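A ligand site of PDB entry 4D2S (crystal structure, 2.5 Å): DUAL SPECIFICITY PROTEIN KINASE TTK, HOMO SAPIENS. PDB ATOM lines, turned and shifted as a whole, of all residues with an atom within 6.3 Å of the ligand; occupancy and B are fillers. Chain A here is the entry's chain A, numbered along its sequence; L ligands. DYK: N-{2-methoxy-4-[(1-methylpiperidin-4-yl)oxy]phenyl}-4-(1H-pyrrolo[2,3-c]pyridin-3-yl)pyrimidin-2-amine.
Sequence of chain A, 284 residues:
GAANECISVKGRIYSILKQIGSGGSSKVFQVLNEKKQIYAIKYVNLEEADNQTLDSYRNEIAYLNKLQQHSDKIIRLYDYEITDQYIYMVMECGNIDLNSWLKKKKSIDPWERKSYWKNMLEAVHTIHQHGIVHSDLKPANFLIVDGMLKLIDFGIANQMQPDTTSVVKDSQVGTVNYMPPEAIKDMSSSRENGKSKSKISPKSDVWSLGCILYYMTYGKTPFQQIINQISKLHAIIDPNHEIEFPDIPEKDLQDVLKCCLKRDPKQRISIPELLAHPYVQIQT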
ATOM      1  N   LYS A  18      29.075  -8.831 -12.115  1.00  0.00           N
ATOM      2  CA  LYS A  18      27.603  -8.712 -12.030  1.00  0.00           C
ATOM      3  C   LYS A  18      27.184  -8.108 -10.670  1.00  0.00           C
ATOM      4  O   LYS A  18      27.991  -8.028  -9.748  1.00  0.00           O
ATOM      5  CB  LYS A  18      26.891 -10.067 -12.291  1.00  0.00           C
ATOM      6  CG  LYS A  18      27.125 -11.163 -11.240  1.00  0.00           C
ATOM      7  CD  LYS A  18      26.134 -12.331 -11.401  1.00  0.00           C
ATOM      8  CE  LYS A  18      25.996 -13.217 -10.186  1.00  0.00           C
ATOM      9  NZ  LYS A  18      27.130 -14.163 -10.034  1.00  0.00           N
ATOM     10  N   GLN A  19      25.908  -7.705 -10.563  1.00  0.00           N
ATOM     11  CA  GLN A  19      25.273  -7.185  -9.362  1.00  0.00           C
ATOM     12  C   GLN A  19      24.627  -8.369  -8.626  1.00  0.00           C
ATOM     13  O   GLN A  19      23.761  -9.056  -9.183  1.00  0.00           O
ATOM     14  CB  GLN A  19      24.240  -6.104  -9.710  1.00  0.00           C
ATOM     15  CG  GLN A  19      23.957  -5.157  -8.547  1.00  0.00           C
ATOM     16  CD  GLN A  19      23.067  -4.003  -8.913  1.00  0.00           C
ATOM     17  OE1 GLN A  19      23.102  -3.471 -10.031  1.00  0.00           O
ATOM     18  NE2 GLN A  19      22.300  -3.532  -7.952  1.00  0.00           N
ATOM     19  N   ILE A  20      25.093  -8.642  -7.395  1.00  0.00           N
ATOM     20  CA  ILE A  20      24.634  -9.751  -6.530  1.00  0.00           C
ATOM     21  C   ILE A  20      23.729  -9.284  -5.362  1.00  0.00           C
ATOM     22  O   ILE A  20      23.191 -10.119  -4.637  1.00  0.00           O
ATOM     23  CB  ILE A  20      25.835 -10.618  -6.013  1.00  0.00           C
ATOM     24  CG1 ILE A  20      26.769  -9.804  -5.074  1.00  0.00           C
ATOM     25  CG2 ILE A  20      26.586 -11.258  -7.183  1.00  0.00           C
ATOM     26  CD1 ILE A  20      28.066 -10.485  -4.590  1.00  0.00           C
ATOM     27  N   GLY A  21      23.583  -7.962  -5.202  1.00  0.00           N
ATOM     28  CA  GLY A  21      22.766  -7.326  -4.158  1.00  0.00           C
ATOM     29  C   GLY A  21      22.341  -5.902  -4.478  1.00  0.00           C
ATOM     30  O   GLY A  21      23.075  -5.161  -5.147  1.00  0.00           O
ATOM     31  N   SER A  22      21.131  -5.518  -4.018  1.00  0.00           N
ATOM     32  CA  SER A  22      20.508  -4.190  -4.199  1.00  0.00           C
ATOM     33  C   SER A  22      19.421  -3.989  -3.133  1.00  0.00           C
ATOM     34  O   SER A  22      18.544  -4.846  -2.988  1.00  0.00           O
ATOM     35  CB  SER A  22      19.895  -4.046  -5.594  1.00  0.00           C
ATOM     36  OG  SER A  22      18.891  -5.015  -5.858  1.00  0.00           O
ATOM     37  N   VAL A  28      25.487  -4.369  -4.144  1.00  0.00           N
ATOM     38  CA  VAL A  28      26.578  -5.306  -3.934  1.00  0.00           C
ATOM     39  C   VAL A  28      26.938  -5.911  -5.305  1.00  0.00           C
ATOM     40  O   VAL A  28      26.054  -6.392  -6.043  1.00  0.00           O
ATOM     41  CB  VAL A  28      26.340  -6.374  -2.812  1.00  0.00           C
ATOM     42  CG1 VAL A  28      27.573  -7.248  -2.585  1.00  0.00           C
ATOM     43  CG2 VAL A  28      25.935  -5.700  -1.495  1.00  0.00           C
ATOM     44  N   GLN A  30      29.771  -8.447  -7.623  1.00  0.00           N
ATOM     45  CA  GLN A  30      30.802  -9.465  -7.714  1.00  0.00           C
ATOM     46  C   GLN A  30      31.816  -8.803  -8.674  1.00  0.00           C
ATOM     47  O   GLN A  30      31.418  -8.301  -9.733  1.00  0.00           O
ATOM     48  CB  GLN A  30      30.264 -10.776  -8.287  1.00  0.00           C
ATOM     49  CG  GLN A  30      31.309 -11.875  -8.268  1.00  0.00           C
ATOM     50  CD  GLN A  30      30.911 -13.081  -9.058  1.00  0.00           C
ATOM     51  OE1 GLN A  30      30.477 -12.984 -10.212  1.00  0.00           O
ATOM     52  NE2 GLN A  30      31.051 -14.251  -8.458  1.00  0.00           N
ATOM     53  N   ALA A  40      33.888  -9.146  -3.431  1.00  0.00           N
ATOM     54  CA  ALA A  40      32.572  -8.527  -3.476  1.00  0.00           C
ATOM     55  C   ALA A  40      32.758  -7.104  -3.022  1.00  0.00           C
ATOM     56  O   ALA A  40      33.581  -6.831  -2.149  1.00  0.00           O
ATOM     57  CB  ALA A  40      31.600  -9.249  -2.569  1.00  0.00           C
ATOM     58  N   LYS A  42      30.553  -3.719  -1.714  1.00  0.00           N
ATOM     59  CA  LYS A  42      29.299  -3.122  -1.280  1.00  0.00           C
ATOM     60  C   LYS A  42      29.440  -1.625  -1.437  1.00  0.00           C
ATOM     61  O   LYS A  42      30.439  -1.029  -1.026  1.00  0.00           O
ATOM     62  CB  LYS A  42      28.945  -3.476   0.171  1.00  0.00           C
ATOM     63  CG  LYS A  42      27.570  -2.957   0.574  1.00  0.00           C
ATOM     64  CD  LYS A  42      27.215  -3.340   2.002  1.00  0.00           C
ATOM     65  CE  LYS A  42      25.821  -2.892   2.343  1.00  0.00           C
ATOM     66  NZ  LYS A  42      25.182  -3.778   3.332  1.00  0.00           N
ATOM     67  N   ILE A  75      32.269 -12.347   7.815  1.00  0.00           N
ATOM     68  CA  ILE A  75      32.672 -11.888   6.469  1.00  0.00           C
ATOM     69  C   ILE A  75      33.990 -11.071   6.518  1.00  0.00           C
ATOM     70  O   ILE A  75      34.128 -10.199   7.351  1.00  0.00           O
ATOM     71  CB  ILE A  75      31.483 -11.099   5.840  1.00  0.00           C
ATOM     72  CG1 ILE A  75      31.738 -10.808   4.343  1.00  0.00           C
ATOM     73  CG2 ILE A  75      31.142  -9.801   6.641  1.00  0.00           C
ATOM     74  CD1 ILE A  75      30.464 -10.550   3.510  1.00  0.00           C
ATOM     75  N   MET A  89      33.032  -0.863   0.345  1.00  0.00           N
ATOM     76  CA  MET A  89      33.555  -1.952   1.183  1.00  0.00           C
ATOM     77  C   MET A  89      33.973  -3.113   0.289  1.00  0.00           C
ATOM     78  O   MET A  89      33.148  -3.665  -0.434  1.00  0.00           O
ATOM     79  CB  MET A  89      32.485  -2.439   2.160  1.00  0.00           C
ATOM     80  CG  MET A  89      32.301  -1.545   3.332  1.00  0.00           C
ATOM     81  SD  MET A  89      30.596  -1.570   3.905  1.00  0.00           S
ATOM     82  CE  MET A  89      30.575  -3.101   4.842  1.00  0.00           C
ATOM     83  N   MET A  91      35.023  -6.795   0.190  1.00  0.00           N
ATOM     84  CA  MET A  91      34.785  -7.996   0.986  1.00  0.00           C
ATOM     85  C   MET A  91      35.103  -9.279   0.264  1.00  0.00           C
ATOM     86  O   MET A  91      35.330  -9.299  -0.959  1.00  0.00           O
ATOM     87  CB  MET A  91      33.305  -8.051   1.418  1.00  0.00           C
ATOM     88  CG  MET A  91      32.840  -6.875   2.252  1.00  0.00           C
ATOM     89  SD  MET A  91      31.040  -6.871   2.467  1.00  0.00           S
ATOM     90  CE  MET A  91      30.509  -6.700   0.763  1.00  0.00           C
ATOM     91  N   GLU A  92      35.078 -10.392   1.028  1.00  0.00           N
ATOM     92  CA  GLU A  92      35.260 -11.719   0.452  1.00  0.00           C
ATOM     93  C   GLU A  92      33.990 -12.080  -0.314  1.00  0.00           C
ATOM     94  O   GLU A  92      32.897 -11.597   0.036  1.00  0.00           O
ATOM     95  CB  GLU A  92      35.635 -12.762   1.522  1.00  0.00           C
ATOM     96  CG  GLU A  92      34.480 -13.304   2.346  1.00  0.00           C
ATOM     97  CD  GLU A  92      34.916 -14.273   3.426  1.00  0.00           C
ATOM     98  OE1 GLU A  92      35.525 -15.317   3.100  1.00  0.00           O
ATOM     99  OE2 GLU A  92      34.637 -13.988   4.617  1.00  0.00           O
ATOM    100  N   CYS A  93      34.132 -12.871  -1.363  1.00  0.00           N
ATOM    101  CA  CYS A  93      32.950 -13.253  -2.087  1.00  0.00           C
ATOM    102  C   CYS A  93      32.452 -14.636  -1.672  1.00  0.00           C
ATOM    103  O   CYS A  93      33.192 -15.626  -1.739  1.00  0.00           O
ATOM    104  CB  CYS A  93      33.180 -13.173  -3.593  1.00  0.00           C
ATOM    105  SG  CYS A  93      31.672 -12.882  -4.548  1.00  0.00           S
ATOM    106  N   GLY A  94      31.202 -14.669  -1.209  1.00  0.00           N
ATOM    107  CA  GLY A  94      30.510 -15.904  -0.878  1.00  0.00           C
ATOM    108  C   GLY A  94      29.845 -16.448  -2.134  1.00  0.00           C
ATOM    109  O   GLY A  94      29.660 -15.705  -3.104  1.00  0.00           O
ATOM    110  N   ASN A  95      29.475 -17.734  -2.133  1.00  0.00           N
ATOM    111  CA  ASN A  95      28.824 -18.369  -3.275  1.00  0.00           C
ATOM    112  C   ASN A  95      27.368 -17.889  -3.377  1.00  0.00           C
ATOM    113  O   ASN A  95      26.895 -17.649  -4.482  1.00  0.00           O
ATOM    114  CB  ASN A  95      28.834 -19.916  -3.161  1.00  0.00           C
ATOM    115  CG  ASN A  95      30.035 -20.614  -2.539  1.00  0.00           C
ATOM    116  OD1 ASN A  95      31.056 -20.011  -2.170  1.00  0.00           O
ATOM    117  ND2 ASN A  95      29.940 -21.914  -2.420  1.00  0.00           N
ATOM    118  N   ILE A  96      26.675 -17.780  -2.227  1.00  0.00           N
ATOM    119  CA  ILE A  96      25.247 -17.419  -2.101  1.00  0.00           C
ATOM    120  C   ILE A  96      24.915 -17.186  -0.613  1.00  0.00           C
ATOM    121  O   ILE A  96      25.631 -17.676   0.254  1.00  0.00           O
ATOM    122  CB  ILE A  96      24.353 -18.572  -2.713  1.00  0.00           C
ATOM    123  CG1 ILE A  96      22.914 -18.091  -3.013  1.00  0.00           C
ATOM    124  CG2 ILE A  96      24.370 -19.869  -1.859  1.00  0.00           C
ATOM    125  CD1 ILE A  96      22.288 -18.669  -4.236  1.00  0.00           C
ATOM    126  N   ASP A  97      23.799 -16.474  -0.335  1.00  0.00           N
ATOM    127  CA  ASP A  97      23.311 -16.255   1.027  1.00  0.00           C
ATOM    128  C   ASP A  97      22.496 -17.479   1.446  1.00  0.00           C
ATOM    129  O   ASP A  97      22.012 -18.213   0.580  1.00  0.00           O
ATOM    130  CB  ASP A  97      22.456 -14.976   1.137  1.00  0.00           C
ATOM    131  CG  ASP A  97      21.131 -15.032   0.400  1.00  0.00           C
ATOM    132  OD1 ASP A  97      21.143 -14.895  -0.847  1.00  0.00           O
ATOM    133  OD2 ASP A  97      20.092 -15.165   1.069  1.00  0.00           O
ATOM    134  N   SER A 100      18.473 -17.772   0.216  1.00  0.00           N
ATOM    135  CA  SER A 100      18.316 -18.208  -1.173  1.00  0.00           C
ATOM    136  C   SER A 100      18.556 -19.710  -1.295  1.00  0.00           C
ATOM    137  O   SER A 100      17.744 -20.400  -1.923  1.00  0.00           O
ATOM    138  CB  SER A 100      19.260 -17.432  -2.076  1.00  0.00           C
ATOM    139  OG  SER A 100      18.978 -16.041  -1.983  1.00  0.00           O
ATOM    140  N   ALA A 140      19.078 -14.468   5.703  1.00  0.00           N
ATOM    141  CA  ALA A 140      19.656 -13.468   4.802  1.00  0.00           C
ATOM    142  C   ALA A 140      20.969 -12.877   5.372  1.00  0.00           C
ATOM    143  O   ALA A 140      21.791 -12.404   4.590  1.00  0.00           O
ATOM    144  CB  ALA A 140      18.660 -12.356   4.561  1.00  0.00           C
ATOM    145  N   LEU A 143      26.040 -15.970   4.922  1.00  0.00           N
ATOM    146  CA  LEU A 143      26.606 -16.208   3.610  1.00  0.00           C
ATOM    147  C   LEU A 143      27.368 -17.528   3.563  1.00  0.00           C
ATOM    148  O   LEU A 143      28.168 -17.808   4.472  1.00  0.00           O
ATOM    149  CB  LEU A 143      27.565 -15.050   3.332  1.00  0.00           C
ATOM    150  CG  LEU A 143      28.172 -14.892   1.950  1.00  0.00           C
ATOM    151  CD1 LEU A 143      27.120 -14.446   0.940  1.00  0.00           C
ATOM    152  CD2 LEU A 143      29.294 -13.890   1.999  1.00  0.00           C
ATOM    153  N   ILE A 144      27.181 -18.314   2.492  1.00  0.00           N
ATOM    154  CA  ILE A 144      27.910 -19.573   2.299  1.00  0.00           C
ATOM    155  C   ILE A 144      29.226 -19.277   1.578  1.00  0.00           C
ATOM    156  O   ILE A 144      29.191 -18.737   0.476  1.00  0.00           O
ATOM    157  CB  ILE A 144      27.041 -20.659   1.604  1.00  0.00           C
ATOM    158  CG1 ILE A 144      25.687 -20.853   2.345  1.00  0.00           C
ATOM    159  CG2 ILE A 144      27.815 -21.993   1.509  1.00  0.00           C
ATOM    160  CD1 ILE A 144      24.716 -21.816   1.765  1.00  0.00           C
ATOM    161  N   ILE A 152      26.970 -11.578   7.838  1.00  0.00           N
ATOM    162  CA  ILE A 152      27.052 -10.431   6.918  1.00  0.00           C
ATOM    163  C   ILE A 152      26.896  -9.079   7.614  1.00  0.00           C
ATOM    164  O   ILE A 152      27.622  -8.132   7.268  1.00  0.00           O
ATOM    165  CB  ILE A 152      26.021 -10.615   5.770  1.00  0.00           C
ATOM    166  CG1 ILE A 152      26.519 -11.607   4.721  1.00  0.00           C
ATOM    167  CG2 ILE A 152      25.596  -9.304   5.118  1.00  0.00           C
ATOM    168  CD1 ILE A 152      25.420 -12.124   3.842  1.00  0.00           C
ATOM    169  N   ASP A 153      25.913  -8.949   8.527  1.00  0.00           N
ATOM    170  CA  ASP A 153      25.715  -7.675   9.235  1.00  0.00           C
ATOM    171  C   ASP A 153      25.462  -7.869  10.744  1.00  0.00           C
ATOM    172  O   ASP A 153      25.377  -9.004  11.231  1.00  0.00           O
ATOM    173  CB  ASP A 153      24.640  -6.799   8.562  1.00  0.00           C
ATOM    174  CG  ASP A 153      23.267  -7.409   8.499  1.00  0.00           C
ATOM    175  OD1 ASP A 153      22.493  -7.232   9.457  1.00  0.00           O
ATOM    176  OD2 ASP A 153      22.943  -8.013   7.462  1.00  0.00           O
HETATM  177  C   DYK L   1      18.205 -14.777  -5.052  1.00  0.00           C
HETATM  178  N   DYK L   1      19.423 -14.014  -5.293  1.00  0.00           N
HETATM  179  O   DYK L   1      23.001 -14.712  -4.806  1.00  0.00           O
HETATM  180  C1  DYK L   1      20.180 -13.833  -4.048  1.00  0.00           C
HETATM  181  N1  DYK L   1      27.928 -13.423  -2.528  1.00  0.00           N
HETATM  182  O1  DYK L   1      27.806 -14.276  -5.053  1.00  0.00           O
HETATM  183  C2  DYK L   1      21.410 -12.950  -4.273  1.00  0.00           C
HETATM  184  N2  DYK L   1      29.456 -12.229  -1.206  1.00  0.00           N
HETATM  185  C3  DYK L   1      22.289 -13.539  -5.361  1.00  0.00           C
HETATM  186  N3  DYK L   1      27.121 -11.665  -1.308  1.00  0.00           N
HETATM  187  C4  DYK L   1      21.510 -13.849  -6.620  1.00  0.00           C
HETATM  188  N4  DYK L   1      24.059  -9.070  -0.043  1.00  0.00           N
HETATM  189  C5  DYK L   1      20.266 -14.686  -6.283  1.00  0.00           C
HETATM  190  N5  DYK L   1      25.221  -6.754   2.625  1.00  0.00           N
HETATM  191  C6  DYK L   1      24.218 -14.399  -4.237  1.00  0.00           C
HETATM  192  C7  DYK L   1      24.267 -13.969  -2.913  1.00  0.00           C
HETATM  193  C8  DYK L   1      25.483 -13.654  -2.333  1.00  0.00           C
HETATM  194  C9  DYK L   1      26.661 -13.738  -3.077  1.00  0.00           C
HETATM  195  C10 DYK L   1      26.592 -14.183  -4.418  1.00  0.00           C
HETATM  196  C11 DYK L   1      25.375 -14.536  -4.986  1.00  0.00           C
HETATM  197  C12 DYK L   1      27.842 -14.869  -6.355  1.00  0.00           C
HETATM  198  C13 DYK L   1      28.198 -12.407  -1.651  1.00  0.00           C
HETATM  199  C14 DYK L   1      29.627 -11.206  -0.356  1.00  0.00           C
HETATM  200  C15 DYK L   1      28.599 -10.382   0.057  1.00  0.00           C
HETATM  201  C16 DYK L   1      27.342 -10.654  -0.453  1.00  0.00           C
HETATM  202  C17 DYK L   1      26.165  -9.860  -0.088  1.00  0.00           C
HETATM  203  C18 DYK L   1      24.902  -9.963  -0.630  1.00  0.00           C
HETATM  204  C19 DYK L   1      24.740  -8.340   0.903  1.00  0.00           C
HETATM  205  C20 DYK L   1      26.070  -8.790   0.918  1.00  0.00           C
HETATM  206  C21 DYK L   1      26.971  -8.203   1.800  1.00  0.00           C
HETATM  207  C22 DYK L   1      26.492  -7.187   2.622  1.00  0.00           C
HETATM  208  C23 DYK L   1      24.360  -7.315   1.767  1.00  0.00           C
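Residues that only touch the ligand: Lys 18 (3.8 Å), Ile 20 (3.4 Å), Val 28 (3.8 Å), Gln 30 (3.9 Å), Ala 40 (3.6 Å), Ile 75 (3.9 Å), Met 91 (3.98 Å), Glu 92 (3.3 Å), Cys 93 (3.7 Å), Asn 95 (3.5 Å), Ile 96 (3.7 Å), Asp 97 (3.5 Å), Ser 100 (3.3 Å), Leu 143 (3.5 Å) and Ile 152 (3.4 Å).
Hydrophobic or aromatic side chains within 4 Å of the ligand: Ile 20, Val 28, Ala 40, Ile 75, Met 91, Ile 96, Leu 143 and Ile 152.
Within 4 Å of the ligand: Lys 18, Ile 20, Val 28, Gln 30, Ala 40, Lys 42, Ile 75, Met 91, Glu 92, Cys 93, Gly 94, Asn 95, Ile 96, Asp 97, Ser 100, Leu 143 and Ile 152.
N of Lys 42 sits at hydrogen-bond distance from O of Met 89, at 2.9 Å.
The side-chain carboxylate (OD1) of Asp 97 is in hydrogen-bond range of the side-chain hydroxyl (OG) of Ser 100, 2.7 Å away.
N of Ile 20 sits at hydrogen-bond distance from O of Val 28, at 2.8 Å.
O of Ile 144 lies within hydrogen-bond range of N of Asn 95, 2.8 Å away.
The backbone carbonyl oxygen of Ala 40 lies within hydrogen-bond range of the backbone NH of Met 91, at 2.7 Å.
O of Ile 96 sits at hydrogen-bond distance from N of Ile 144 (2.8 Å).
The backbone NH (N) of Val 28 lies within hydrogen-bond range of the backbone carbonyl oxygen (O) of Gly 21, 2.7 Å away.
O of Lys 18 is in hydrogen-bond range of N of Gln 30, at 2.8 Å.
A nitrogen (N2) of the ligand lies within hydrogen-bond range of the backbone NH (N) of Gly 94, at 3.0 Å.
O of Gly 94 is in hydrogen-bond range of N1 of the ligand (2.9 Å).
A nitrogen (N5) of the ligand lies within hydrogen-bond range of the side-chain amino group of Lys 42 (3.1 Å).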
